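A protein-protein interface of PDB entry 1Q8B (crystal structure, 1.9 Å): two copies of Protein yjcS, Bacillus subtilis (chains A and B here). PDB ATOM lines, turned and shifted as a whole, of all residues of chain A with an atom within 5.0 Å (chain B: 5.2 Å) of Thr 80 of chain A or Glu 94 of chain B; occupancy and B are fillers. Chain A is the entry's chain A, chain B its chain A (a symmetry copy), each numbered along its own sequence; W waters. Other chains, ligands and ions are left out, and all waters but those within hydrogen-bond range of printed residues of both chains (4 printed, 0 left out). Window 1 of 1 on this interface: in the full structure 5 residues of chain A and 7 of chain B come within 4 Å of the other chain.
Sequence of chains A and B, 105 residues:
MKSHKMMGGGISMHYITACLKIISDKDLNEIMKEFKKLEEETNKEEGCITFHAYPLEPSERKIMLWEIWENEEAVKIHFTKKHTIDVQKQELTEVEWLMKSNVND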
ATOM      1  N   LYS A  76     -17.339 -17.760   1.351  1.00  0.00           N
ATOM      2  CA  LYS A  76     -17.804 -18.385   0.124  1.00  0.00           C
ATOM      3  C   LYS A  76     -17.312 -19.828   0.041  1.00  0.00           C
ATOM      4  O   LYS A  76     -18.069 -20.720  -0.336  1.00  0.00           O
ATOM      5  CB  LYS A  76     -17.338 -17.566  -1.084  1.00  0.00           C
ATOM      6  CG  LYS A  76     -18.112 -16.258  -1.209  1.00  0.00           C
ATOM      7  CD  LYS A  76     -17.554 -15.316  -2.259  1.00  0.00           C
ATOM      8  CE  LYS A  76     -18.429 -14.071  -2.353  1.00  0.00           C
ATOM      9  NZ  LYS A  76     -17.832 -13.016  -3.219  1.00  0.00           N
ATOM     10  N   ILE A  77     -16.050 -20.054   0.404  1.00  0.00           N
ATOM     11  CA  ILE A  77     -15.482 -21.407   0.397  1.00  0.00           C
ATOM     12  C   ILE A  77     -16.300 -22.285   1.343  1.00  0.00           C
ATOM     13  O   ILE A  77     -16.582 -23.449   1.047  1.00  0.00           O
ATOM     14  CB  ILE A  77     -14.000 -21.396   0.845  1.00  0.00           C
ATOM     15  CG1 ILE A  77     -13.122 -20.872  -0.293  1.00  0.00           C
ATOM     16  CG2 ILE A  77     -13.558 -22.790   1.244  1.00  0.00           C
ATOM     17  CD1 ILE A  77     -11.683 -20.653   0.087  1.00  0.00           C
ATOM     18  N   HIS A  78     -16.677 -21.709   2.480  1.00  0.00           N
ATOM     19  CA  HIS A  78     -17.489 -22.396   3.475  1.00  0.00           C
ATOM     20  C   HIS A  78     -18.758 -22.990   2.859  1.00  0.00           C
ATOM     21  O   HIS A  78     -19.136 -24.119   3.175  1.00  0.00           O
ATOM     22  CB  HIS A  78     -17.876 -21.408   4.582  1.00  0.00           C
ATOM     23  CG  HIS A  78     -18.979 -21.885   5.480  1.00  0.00           C
ATOM     24  ND1 HIS A  78     -18.890 -23.038   6.231  1.00  0.00           N
ATOM     25  CD2 HIS A  78     -20.183 -21.340   5.773  1.00  0.00           C
ATOM     26  CE1 HIS A  78     -19.990 -23.182   6.949  1.00  0.00           C
ATOM     27  NE2 HIS A  78     -20.792 -22.164   6.690  1.00  0.00           N
ATOM     28  N   PHE A  79     -19.415 -22.232   1.986  1.00  0.00           N
ATOM     29  CA  PHE A  79     -20.647 -22.714   1.380  1.00  0.00           C
ATOM     30  C   PHE A  79     -20.464 -23.718   0.256  1.00  0.00           C
ATOM     31  O   PHE A  79     -21.450 -24.189  -0.309  1.00  0.00           O
ATOM     32  CB  PHE A  79     -21.510 -21.544   0.902  1.00  0.00           C
ATOM     33  CG  PHE A  79     -22.058 -20.722   2.020  1.00  0.00           C
ATOM     34  CD1 PHE A  79     -21.468 -19.515   2.368  1.00  0.00           C
ATOM     35  CD2 PHE A  79     -23.127 -21.189   2.779  1.00  0.00           C
ATOM     36  CE1 PHE A  79     -21.932 -18.785   3.463  1.00  0.00           C
ATOM     37  CE2 PHE A  79     -23.598 -20.464   3.878  1.00  0.00           C
ATOM     38  CZ  PHE A  79     -22.996 -19.262   4.217  1.00  0.00           C
ATOM     39  N   THR A  80     -19.215 -24.048  -0.073  1.00  0.00           N
ATOM     40  CA  THR A  80     -18.959 -25.045  -1.108  1.00  0.00           C
ATOM     41  C   THR A  80     -18.664 -26.382  -0.427  1.00  0.00           C
ATOM     42  O   THR A  80     -18.726 -27.436  -1.056  1.00  0.00           O
ATOM     43  CB  THR A  80     -17.755 -24.676  -1.994  1.00  0.00           C
ATOM     44  OG1 THR A  80     -16.544 -24.818  -1.242  1.00  0.00           O
ATOM     45  CG2 THR A  80     -17.878 -23.251  -2.501  1.00  0.00           C
ATOM     46  N   LYS A  81     -18.347 -26.331   0.865  1.00  0.00           N
ATOM     47  CA  LYS A  81     -18.044 -27.535   1.634  1.00  0.00           C
ATOM     48  C   LYS A  81     -19.272 -28.430   1.698  1.00  0.00           C
ATOM     49  O   LYS A  81     -20.396 -27.941   1.811  1.00  0.00           O
ATOM     50  CB  LYS A  81     -17.633 -27.168   3.058  1.00  0.00           C
ATOM     51  CG  LYS A  81     -16.483 -26.188   3.157  1.00  0.00           C
ATOM     52  CD  LYS A  81     -15.217 -26.761   2.574  1.00  0.00           C
ATOM     53  CE  LYS A  81     -14.048 -25.851   2.874  1.00  0.00           C
ATOM     54  NZ  LYS A  81     -12.786 -26.366   2.271  1.00  0.00           N
ATOM     55  N   LYS A  82     -19.059 -29.739   1.638  1.00  0.00           N
ATOM     56  CA  LYS A  82     -20.165 -30.682   1.688  1.00  0.00           C
ATOM     57  C   LYS A  82     -20.889 -30.667   3.032  1.00  0.00           C
ATOM     58  O   LYS A  82     -22.103 -30.844   3.077  1.00  0.00           O
ATOM     59  CB  LYS A  82     -19.678 -32.103   1.401  1.00  0.00           C
ATOM     60  CG  LYS A  82     -20.790 -33.132   1.520  1.00  0.00           C
ATOM     61  CD  LYS A  82     -20.289 -34.566   1.455  1.00  0.00           C
ATOM     62  CE  LYS A  82     -21.463 -35.533   1.563  1.00  0.00           C
ATOM     63  NZ  LYS A  82     -22.453 -35.260   0.469  1.00  0.00           N
ATOM     64  N   ILE A  85     -23.324 -27.775   2.767  1.00  0.00           N
ATOM     65  CA  ILE A  85     -24.417 -28.073   1.844  1.00  0.00           C
ATOM     66  C   ILE A  85     -25.369 -29.140   2.396  1.00  0.00           C
ATOM     67  O   ILE A  85     -26.574 -29.095   2.140  1.00  0.00           O
ATOM     68  CB  ILE A  85     -23.863 -28.521   0.473  1.00  0.00           C
ATOM     69  CG1 ILE A  85     -23.090 -27.367  -0.165  1.00  0.00           C
ATOM     70  CG2 ILE A  85     -24.996 -28.957  -0.436  1.00  0.00           C
ATOM     71  CD1 ILE A  85     -22.293 -27.761  -1.394  1.00  0.00           C
ATOM     72  N   CYS B  19      -8.321 -24.034  -6.070  1.00  0.00           N
ATOM     73  CA  CYS B  19      -7.940 -25.427  -6.010  1.00  0.00           C
ATOM     74  C   CYS B  19      -9.136 -26.147  -5.435  1.00  0.00           C
ATOM     75  O   CYS B  19      -9.599 -25.809  -4.344  1.00  0.00           O
ATOM     76  CB  CYS B  19      -6.738 -25.633  -5.091  1.00  0.00           C
ATOM     77  SG  CYS B  19      -6.207 -27.373  -5.000  1.00  0.00           S
ATOM     78  N   LEU B  20      -9.640 -27.126  -6.177  1.00  0.00           N
ATOM     79  CA  LEU B  20     -10.785 -27.906  -5.744  1.00  0.00           C
ATOM     80  C   LEU B  20     -10.356 -29.256  -5.186  1.00  0.00           C
ATOM     81  O   LEU B  20      -9.466 -29.916  -5.726  1.00  0.00           O
ATOM     82  CB  LEU B  20     -11.740 -28.168  -6.910  1.00  0.00           C
ATOM     83  CG  LEU B  20     -12.311 -27.018  -7.739  1.00  0.00           C
ATOM     84  CD1 LEU B  20     -13.357 -27.579  -8.687  1.00  0.00           C
ATOM     85  CD2 LEU B  20     -12.934 -25.970  -6.837  1.00  0.00           C
ATOM     86  N   LYS B  21     -10.997 -29.663  -4.100  1.00  0.00           N
ATOM     87  CA  LYS B  21     -10.721 -30.958  -3.513  1.00  0.00           C
ATOM     88  C   LYS B  21     -11.819 -31.891  -4.037  1.00  0.00           C
ATOM     89  O   LYS B  21     -13.004 -31.568  -3.937  1.00  0.00           O
ATOM     90  CB  LYS B  21     -10.786 -30.872  -1.987  1.00  0.00           C
ATOM     91  CG  LYS B  21     -10.364 -32.155  -1.296  1.00  0.00           C
ATOM     92  CD  LYS B  21     -10.781 -32.160   0.152  1.00  0.00           C
ATOM     93  CE  LYS B  21     -10.551 -33.528   0.752  1.00  0.00           C
ATOM     94  NZ  LYS B  21     -11.122 -33.609   2.121  1.00  0.00           N
ATOM     95  N   ILE B  23     -14.226 -34.774  -3.696  1.00  0.00           N
ATOM     96  CA  ILE B  23     -14.812 -35.539  -2.602  1.00  0.00           C
ATOM     97  C   ILE B  23     -15.569 -36.745  -3.147  1.00  0.00           C
ATOM     98  O   ILE B  23     -16.086 -37.565  -2.391  1.00  0.00           O
ATOM     99  CB  ILE B  23     -15.752 -34.655  -1.753  1.00  0.00           C
ATOM    100  CG1 ILE B  23     -16.844 -34.041  -2.635  1.00  0.00           C
ATOM    101  CG2 ILE B  23     -14.936 -33.562  -1.062  1.00  0.00           C
ATOM    102  CD1 ILE B  23     -17.772 -33.085  -1.892  1.00  0.00           C
ATOM    103  N   LEU B  92     -19.113 -33.322  -6.918  1.00  0.00           N
ATOM    104  CA  LEU B  92     -17.833 -33.967  -7.174  1.00  0.00           C
ATOM    105  C   LEU B  92     -16.691 -33.312  -6.413  1.00  0.00           C
ATOM    106  O   LEU B  92     -15.690 -33.959  -6.106  1.00  0.00           O
ATOM    107  CB  LEU B  92     -17.525 -33.918  -8.667  1.00  0.00           C
ATOM    108  CG  LEU B  92     -18.564 -34.561  -9.588  1.00  0.00           C
ATOM    109  CD1 LEU B  92     -18.290 -34.167 -11.040  1.00  0.00           C
ATOM    110  CD2 LEU B  92     -18.534 -36.076  -9.395  1.00  0.00           C
ATOM    111  N   THR B  93     -16.854 -32.029  -6.101  1.00  0.00           N
ATOM    112  CA  THR B  93     -15.810 -31.271  -5.417  1.00  0.00           C
ATOM    113  C   THR B  93     -16.331 -30.255  -4.403  1.00  0.00           C
ATOM    114  O   THR B  93     -17.532 -30.083  -4.211  1.00  0.00           O
ATOM    115  CB  THR B  93     -14.986 -30.438  -6.435  1.00  0.00           C
ATOM    116  OG1 THR B  93     -15.864 -29.517  -7.102  1.00  0.00           O
ATOM    117  CG2 THR B  93     -14.325 -31.330  -7.478  1.00  0.00           C
ATOM    118  N   GLU B  94     -15.377 -29.592  -3.763  1.00  0.00           N
ATOM    119  CA  GLU B  94     -15.620 -28.504  -2.827  1.00  0.00           C
ATOM    120  C   GLU B  94     -14.338 -27.686  -2.960  1.00  0.00           C
ATOM    121  O   GLU B  94     -13.284 -28.241  -3.285  1.00  0.00           O
ATOM    122  CB  GLU B  94     -15.835 -29.003  -1.383  1.00  0.00           C
ATOM    123  CG  GLU B  94     -14.715 -29.792  -0.754  1.00  0.00           C
ATOM    124  CD  GLU B  94     -15.051 -30.218   0.665  1.00  0.00           C
ATOM    125  OE1 GLU B  94     -16.238 -30.489   0.946  1.00  0.00           O
ATOM    126  OE2 GLU B  94     -14.133 -30.299   1.502  1.00  0.00           O
ATOM    127  N   VAL B  95     -14.427 -26.375  -2.766  1.00  0.00           N
ATOM    128  CA  VAL B  95     -13.251 -25.517  -2.883  1.00  0.00           C
ATOM    129  C   VAL B  95     -12.384 -25.625  -1.633  1.00  0.00           C
ATOM    130  O   VAL B  95     -12.872 -25.463  -0.517  1.00  0.00           O
ATOM    131  CB  VAL B  95     -13.656 -24.037  -3.088  1.00  0.00           C
ATOM    132  CG1 VAL B  95     -12.420 -23.155  -3.144  1.00  0.00           C
ATOM    133  CG2 VAL B  95     -14.456 -23.897  -4.363  1.00  0.00           C
ATOM    134  N   GLU B  96     -11.101 -25.914  -1.828  1.00  0.00           N
ATOM    135  CA  GLU B  96     -10.167 -26.033  -0.716  1.00  0.00           C
ATOM    136  C   GLU B  96      -9.602 -24.645  -0.423  1.00  0.00           C
ATOM    137  O   GLU B  96      -9.534 -24.221   0.729  1.00  0.00           O
ATOM    138  CB  GLU B  96      -9.041 -27.008  -1.063  1.00  0.00           C
ATOM    139  CG  GLU B  96      -8.243 -27.448   0.147  1.00  0.00           C
ATOM    140  CD  GLU B  96      -7.234 -28.526  -0.180  1.00  0.00           C
ATOM    141  OE1 GLU B  96      -6.192 -28.209  -0.797  1.00  0.00           O
ATOM    142  OE2 GLU B  96      -7.490 -29.697   0.176  1.00  0.00           O
HETATM  143  O   HOH W   1     -17.133 -31.147   3.664  1.00  0.00           O
HETATM  144  O   HOH W   2     -12.031 -28.801   1.471  1.00  0.00           O
HETATM  145  O   HOH W   3     -10.746 -24.661   3.009  1.00  0.00           O
HETATM  146  O   HOH W   4     -19.130 -30.094  -1.947  1.00  0.00           O
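OG1 of Thr 80 of chain A lies within hydrogen-bond range of N of Val 95 of chain B (3.0 Å). NZ of Lys 81 of chain A sits at hydrogen-bond distance from O of Val 95 of chain B (2.9 Å). The backbone NH (N) of Lys 82 of chain A lies within hydrogen-bond range of the side-chain carboxylate (OE1) of Glu 94 of chain B, 3.0 Å away.
The side-chain hydroxyl (OG1) of Thr 80 of chain A lies within hydrogen-bond range of the backbone carbonyl oxygen (O) of Ile 77 of chain A (2.7 Å). The backbone carbonyl oxygen (O) of Cys 19 of chain B sits at hydrogen-bond distance from the backbone NH (N) of Glu 96 of chain B (2.9 Å). The backbone carbonyl oxygen of Glu 94 of chain B lies within hydrogen-bond range of the backbone NH of Lys 21 of chain B. The backbone NH of Ile 23 of chain B is in hydrogen-bond range of the backbone carbonyl oxygen of Leu 92 of chain B (2.9 Å).
Val 95 of chain B touches Ile 77 of chain A (O to CG2, 3.3 Å). Glu 94 of chain B touches Thr 80 of chain A. CA of Lys 81 of chain A touches OE1 of Glu 94 of chain B, at 3.5 Å. Lys 81 of chain A touches Glu 96 of chain B. Lys 82 of chain A touches Ile 23 of chain B.
Printed residues of chain B within 4 Å of Thr 80 of chain A: Glu 94 (3.3 Å) and Val 95 (3.0 Å). Printed residues of chain B within 4 Å of Lys 81 of chain A: Glu 94, Val 95 and Glu 96. Of chain A, only Thr 80 (3.3 Å), Lys 81 (3.5 Å) and Lys 82 (3.0 Å) come within 4 Å of Glu 94 of chain B. Of the printed residues of chain A, Val 95 of chain B touches Ile 77 (3.3 Å), Thr 80 (3.0 Å) and Lys 81 (2.9 Å). The nearest residue of chain B that does not touch Thr 80 of chain A is Thr 93 of chain B (4.3 Å).
Printed residues of chain A that touch a printed residue of chain B: Ile 77, Thr 80, Lys 81 and Lys 82. Hydrophobic or aromatic side chains of chain A within 4 Å of the printed part of chain B: Ile 77. Along chain A the printed residues that touch a printed residue of chain B span positions 77 to 82. Hydrophobic or aromatic side chains of chain B that line the printed part of chain A: Ile 23 and Val 95. Among the printed residues, no Asp or Glu carboxylate lies within 4 Å of a Lys or Arg side-chain nitrogen of the other chain.
No position is printed for both chains. Of the 8 pairs that touch across the chains among the printed residues, none has its exchanged pair printed and touching as well.
Water W2 lies within hydrogen-bond range of the side-chain carboxylate (OE2) of Glu 94 of chain B (2.6 Å) and the side-chain amino group (NZ) of Lys 81 of chain A (2.7 Å). Water W3 lies within hydrogen-bond range of O of Glu 96 of chain B (2.6 Å) and NZ of Lys 81 of chain A (2.8 Å). Water W4 lies within hydrogen-bond range of the backbone carbonyl oxygen of Thr 93 of chain B (2.8 Å) and the backbone carbonyl oxygen of Thr 80 of chain A (2.8 Å). Water W1 bridges OE1 of Glu 94 of chain B (2.9 Å) and N of Lys 82 of chain A (3.1 Å).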
